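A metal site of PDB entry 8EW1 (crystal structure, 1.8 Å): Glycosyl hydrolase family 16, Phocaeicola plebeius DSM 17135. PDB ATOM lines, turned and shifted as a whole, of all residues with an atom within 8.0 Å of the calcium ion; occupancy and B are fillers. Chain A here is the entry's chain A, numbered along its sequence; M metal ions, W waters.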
ATOM      1  N   ASP A  45     -24.031   4.656 -23.585  1.00  0.00           N
ATOM      2  CA  ASP A  45     -22.602   4.358 -23.637  1.00  0.00           C
ATOM      3  C   ASP A  45     -22.316   3.464 -24.831  1.00  0.00           C
ATOM      4  O   ASP A  45     -22.847   2.347 -24.917  1.00  0.00           O
ATOM      5  CB  ASP A  45     -22.130   3.683 -22.346  1.00  0.00           C
ATOM      6  CG  ASP A  45     -20.627   3.843 -22.103  1.00  0.00           C
ATOM      7  OD1 ASP A  45     -19.873   3.945 -23.091  1.00  0.00           O
ATOM      8  OD2 ASP A  45     -20.214   3.851 -20.929  1.00  0.00           O
ATOM      9  N   GLU A  46     -21.484   3.944 -25.742  1.00  0.00           N
ATOM     10  CA  GLU A  46     -21.043   3.139 -26.879  1.00  0.00           C
ATOM     11  C   GLU A  46     -19.821   2.295 -26.563  1.00  0.00           C
ATOM     12  O   GLU A  46     -19.367   1.530 -27.423  1.00  0.00           O
ATOM     13  CB  GLU A  46     -20.761   4.057 -28.079  1.00  0.00           C
ATOM     14  CG  GLU A  46     -21.974   4.867 -28.517  1.00  0.00           C
ATOM     15  CD  GLU A  46     -23.137   3.994 -28.995  1.00  0.00           C
ATOM     16  OE1 GLU A  46     -22.913   3.116 -29.849  1.00  0.00           O
ATOM     17  OE2 GLU A  46     -24.270   4.197 -28.506  1.00  0.00           O
ATOM     18  N   PHE A  47     -19.265   2.433 -25.356  1.00  0.00           N
ATOM     19  CA  PHE A  47     -18.148   1.619 -24.881  1.00  0.00           C
ATOM     20  C   PHE A  47     -16.940   1.676 -25.812  1.00  0.00           C
ATOM     21  O   PHE A  47     -16.289   0.665 -26.076  1.00  0.00           O
ATOM     22  CB  PHE A  47     -18.590   0.175 -24.626  1.00  0.00           C
ATOM     23  CG  PHE A  47     -19.573   0.043 -23.495  1.00  0.00           C
ATOM     24  CD1 PHE A  47     -19.214   0.419 -22.202  1.00  0.00           C
ATOM     25  CD2 PHE A  47     -20.853  -0.430 -23.713  1.00  0.00           C
ATOM     26  CE1 PHE A  47     -20.104   0.312 -21.160  1.00  0.00           C
ATOM     27  CE2 PHE A  47     -21.752  -0.549 -22.669  1.00  0.00           C
ATOM     28  CZ  PHE A  47     -21.382  -0.176 -21.395  1.00  0.00           C
ATOM     29  N   LYS A  48     -16.633   2.865 -26.305  1.00  0.00           N
ATOM     30  CA  LYS A  48     -15.385   3.044 -27.043  1.00  0.00           C
ATOM     31  C   LYS A  48     -14.220   3.252 -26.074  1.00  0.00           C
ATOM     32  O   LYS A  48     -14.402   3.475 -24.875  1.00  0.00           O
ATOM     33  CB  LYS A  48     -15.499   4.229 -28.004  1.00  0.00           C
ATOM     34  CG  LYS A  48     -16.553   4.062 -29.095  1.00  0.00           C
ATOM     35  CD  LYS A  48     -16.634   5.307 -29.970  1.00  0.00           C
ATOM     36  CE  LYS A  48     -18.040   5.498 -30.522  1.00  0.00           C
ATOM     37  NZ  LYS A  48     -18.433   4.381 -31.421  1.00  0.00           N
ATOM     38  N   GLY A  49     -13.014   3.173 -26.614  1.00  0.00           N
ATOM     39  CA  GLY A  49     -11.821   3.440 -25.826  1.00  0.00           C
ATOM     40  C   GLY A  49     -11.295   2.226 -25.089  1.00  0.00           C
ATOM     41  O   GLY A  49     -11.531   1.077 -25.471  1.00  0.00           O
ATOM     42  N   GLU A  80     -12.540  -3.307 -25.149  1.00  0.00           N
ATOM     43  CA  GLU A  80     -11.745  -3.661 -26.320  1.00  0.00           C
ATOM     44  C   GLU A  80     -12.597  -3.586 -27.578  1.00  0.00           C
ATOM     45  O   GLU A  80     -13.728  -4.099 -27.610  1.00  0.00           O
ATOM     46  CB  GLU A  80     -11.153  -5.071 -26.155  1.00  0.00           C
ATOM     47  CG  GLU A  80     -10.410  -5.262 -24.847  1.00  0.00           C
ATOM     48  CD  GLU A  80     -10.335  -6.704 -24.382  1.00  0.00           C
ATOM     49  OE1 GLU A  80     -10.666  -7.620 -25.164  1.00  0.00           O
ATOM     50  OE2 GLU A  80      -9.973  -6.925 -23.208  1.00  0.00           O
ATOM     51  N   ASP A  81     -12.048  -2.949 -28.609  1.00  0.00           N
ATOM     52  CA  ASP A  81     -12.643  -2.925 -29.947  1.00  0.00           C
ATOM     53  C   ASP A  81     -14.073  -2.397 -29.899  1.00  0.00           C
ATOM     54  O   ASP A  81     -14.965  -2.899 -30.583  1.00  0.00           O
ATOM     55  CB  ASP A  81     -12.585  -4.291 -30.615  1.00  0.00           C
ATOM     56  CG  ASP A  81     -12.988  -4.261 -32.084  1.00  0.00           C
ATOM     57  OD1 ASP A  81     -12.299  -3.566 -32.869  1.00  0.00           O
ATOM     58  OD2 ASP A  81     -13.993  -4.899 -32.455  1.00  0.00           O
ATOM     59  N   GLY A  82     -14.297  -1.364 -29.082  1.00  0.00           N
ATOM     60  CA  GLY A  82     -15.615  -0.758 -28.966  1.00  0.00           C
ATOM     61  C   GLY A  82     -16.631  -1.569 -28.213  1.00  0.00           C
ATOM     62  O   GLY A  82     -17.832  -1.318 -28.353  1.00  0.00           O
ATOM     63  N   CYS A  83     -16.201  -2.533 -27.404  1.00  0.00           N
ATOM     64  CA  CYS A  83     -17.114  -3.331 -26.590  1.00  0.00           C
ATOM     65  C   CYS A  83     -16.617  -3.383 -25.156  1.00  0.00           C
ATOM     66  O   CYS A  83     -15.415  -3.412 -24.893  1.00  0.00           O
ATOM     67  CB  CYS A  83     -17.253  -4.760 -27.112  1.00  0.00           C
ATOM     68  SG  CYS A  83     -18.203  -4.924 -28.626  1.00  0.00           S
ATOM     69  N   CYS A  84     -17.579  -3.411 -24.237  1.00  0.00           N
ATOM     70  CA  CYS A  84     -17.318  -3.839 -22.870  1.00  0.00           C
ATOM     71  C   CYS A  84     -17.219  -5.365 -22.854  1.00  0.00           C
ATOM     72  O   CYS A  84     -18.099  -6.048 -23.385  1.00  0.00           O
ATOM     73  CB  CYS A  84     -18.422  -3.359 -21.931  1.00  0.00           C
ATOM     74  SG  CYS A  84     -18.291  -3.961 -20.242  1.00  0.00           S
ATOM     75  N   ARG A 121     -26.990  -4.041 -27.098  1.00  0.00           N
ATOM     76  CA  ARG A 121     -26.521  -5.006 -28.085  1.00  0.00           C
ATOM     77  C   ARG A 121     -25.506  -5.919 -27.417  1.00  0.00           C
ATOM     78  O   ARG A 121     -24.464  -5.442 -26.934  1.00  0.00           O
ATOM     79  CB  ARG A 121     -25.925  -4.307 -29.307  1.00  0.00           C
ATOM     80  CG  ARG A 121     -25.549  -5.232 -30.441  1.00  0.00           C
ATOM     81  CD  ARG A 121     -25.372  -4.465 -31.749  1.00  0.00           C
ATOM     82  NE  ARG A 121     -25.148  -5.355 -32.870  1.00  0.00           N
ATOM     83  CZ  ARG A 121     -23.951  -5.717 -33.319  1.00  0.00           C
ATOM     84  NH1 ARG A 121     -22.841  -5.243 -32.757  1.00  0.00           N
ATOM     85  NH2 ARG A 121     -23.859  -6.580 -34.324  1.00  0.00           N
ATOM     86  N   PHE A 198     -24.264 -11.284 -32.040  1.00  0.00           N
ATOM     87  CA  PHE A 198     -24.856 -10.161 -31.323  1.00  0.00           C
ATOM     88  C   PHE A 198     -26.362 -10.131 -31.545  1.00  0.00           C
ATOM     89  O   PHE A 198     -26.853 -10.450 -32.636  1.00  0.00           O
ATOM     90  CB  PHE A 198     -24.244  -8.842 -31.800  1.00  0.00           C
ATOM     91  CG  PHE A 198     -22.926  -8.503 -31.166  1.00  0.00           C
ATOM     92  CD1 PHE A 198     -22.886  -7.824 -29.967  1.00  0.00           C
ATOM     93  CD2 PHE A 198     -21.727  -8.846 -31.780  1.00  0.00           C
ATOM     94  CE1 PHE A 198     -21.675  -7.484 -29.377  1.00  0.00           C
ATOM     95  CE2 PHE A 198     -20.512  -8.528 -31.196  1.00  0.00           C
ATOM     96  CZ  PHE A 198     -20.484  -7.838 -29.989  1.00  0.00           C
ATOM     97  N   ILE A 258     -20.658  -6.446 -24.664  1.00  0.00           N
ATOM     98  CA  ILE A 258     -21.696  -5.427 -24.727  1.00  0.00           C
ATOM     99  C   ILE A 258     -21.209  -4.340 -25.672  1.00  0.00           C
ATOM    100  O   ILE A 258     -20.264  -3.603 -25.362  1.00  0.00           O
ATOM    101  CB  ILE A 258     -22.009  -4.839 -23.341  1.00  0.00           C
ATOM    102  CG1 ILE A 258     -22.335  -5.958 -22.341  1.00  0.00           C
ATOM    103  CG2 ILE A 258     -23.171  -3.857 -23.438  1.00  0.00           C
ATOM    104  CD1 ILE A 258     -21.147  -6.392 -21.520  1.00  0.00           C
ATOM    105  N   ASP A 259     -21.847  -4.252 -26.849  1.00  0.00           N
ATOM    106  CA  ASP A 259     -21.476  -3.245 -27.838  1.00  0.00           C
ATOM    107  C   ASP A 259     -21.928  -1.859 -27.397  1.00  0.00           C
ATOM    108  O   ASP A 259     -21.169  -0.889 -27.516  1.00  0.00           O
ATOM    109  CB  ASP A 259     -22.085  -3.603 -29.191  1.00  0.00           C
ATOM    110  CG  ASP A 259     -21.601  -2.692 -30.314  1.00  0.00           C
ATOM    111  OD1 ASP A 259     -20.636  -1.922 -30.101  1.00  0.00           O
ATOM    112  OD2 ASP A 259     -22.197  -2.756 -31.414  1.00  0.00           O
ATOM    113  N   TYR A 260     -23.156  -1.734 -26.903  1.00  0.00           N
ATOM    114  CA  TYR A 260     -23.647  -0.443 -26.453  1.00  0.00           C
ATOM    115  C   TYR A 260     -24.822  -0.646 -25.508  1.00  0.00           C
ATOM    116  O   TYR A 260     -25.455  -1.716 -25.483  1.00  0.00           O
ATOM    117  CB  TYR A 260     -24.075   0.457 -27.620  1.00  0.00           C
ATOM    118  CG  TYR A 260     -25.285  -0.018 -28.396  1.00  0.00           C
ATOM    119  CD1 TYR A 260     -26.559   0.110 -27.873  1.00  0.00           C
ATOM    120  CD2 TYR A 260     -25.160  -0.564 -29.671  1.00  0.00           C
ATOM    121  CE1 TYR A 260     -27.671  -0.302 -28.571  1.00  0.00           C
ATOM    122  CE2 TYR A 260     -26.259  -0.970 -30.383  1.00  0.00           C
ATOM    123  CZ  TYR A 260     -27.522  -0.838 -29.833  1.00  0.00           C
ATOM    124  OH  TYR A 260     -28.639  -1.244 -30.519  1.00  0.00           O
ATOM    125  N   VAL A 261     -25.093   0.397 -24.731  1.00  0.00           N
ATOM    126  CA  VAL A 261     -26.340   0.556 -23.980  1.00  0.00           C
ATOM    127  C   VAL A 261     -26.881   1.937 -24.326  1.00  0.00           C
ATOM    128  O   VAL A 261     -26.174   2.943 -24.159  1.00  0.00           O
ATOM    129  CB  VAL A 261     -26.114   0.435 -22.459  1.00  0.00           C
ATOM    130  CG1 VAL A 261     -27.391   0.805 -21.690  1.00  0.00           C
ATOM    131  CG2 VAL A 261     -25.648  -0.969 -22.108  1.00  0.00           C
ATOM    132  N   ARG A 262     -28.116   1.993 -24.814  1.00  0.00           N
ATOM    133  CA  ARG A 262     -28.733   3.242 -25.230  1.00  0.00           C
ATOM    134  C   ARG A 262     -30.037   3.454 -24.468  1.00  0.00           C
ATOM    135  O   ARG A 262     -30.801   2.511 -24.239  1.00  0.00           O
ATOM    136  CB  ARG A 262     -28.984   3.260 -26.731  1.00  0.00           C
ATOM    137  CG  ARG A 262     -27.700   3.294 -27.555  1.00  0.00           C
ATOM    138  CD  ARG A 262     -27.941   3.148 -29.043  1.00  0.00           C
ATOM    139  NE  ARG A 262     -26.693   3.042 -29.786  1.00  0.00           N
ATOM    140  CZ  ARG A 262     -26.575   2.585 -31.029  1.00  0.00           C
ATOM    141  NH1 ARG A 262     -27.627   2.175 -31.713  1.00  0.00           N
ATOM    142  NH2 ARG A 262     -25.368   2.529 -31.587  1.00  0.00           N
HETATM  143 CA    CA M   1     -19.688  -0.085 -29.160  1.00  0.00          CA
HETATM  144  O   HOH W   1     -21.347   0.973 -30.173  1.00  0.00           O
HETATM  145  O   HOH W   2     -18.667  -0.623 -31.397  1.00  0.00           O
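The side-chain carboxylate (OE2) of Glu 46 lies within salt-bridge range of the guanidinium group (NE) of Arg 262 (3.0 Å).
The side-chain carboxylate (OD2) of Asp 259 is in salt-bridge range of the guanidinium group (NH1) of Arg 121 (2.9 Å).
Of the 17 residues printed, 3 come within 4 Å of the calcium ion.
The calcium ion is bound by water W1 (2.2 Å), OD1 of Asp 259 (2.3 Å), O of Asp 259 (2.4 Å), O of Gly 82 (2.4 Å), O of Glu 46 (2.4 Å) and water W2 (2.5 Å).
The calcium ion has six donor atoms within binding distance.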
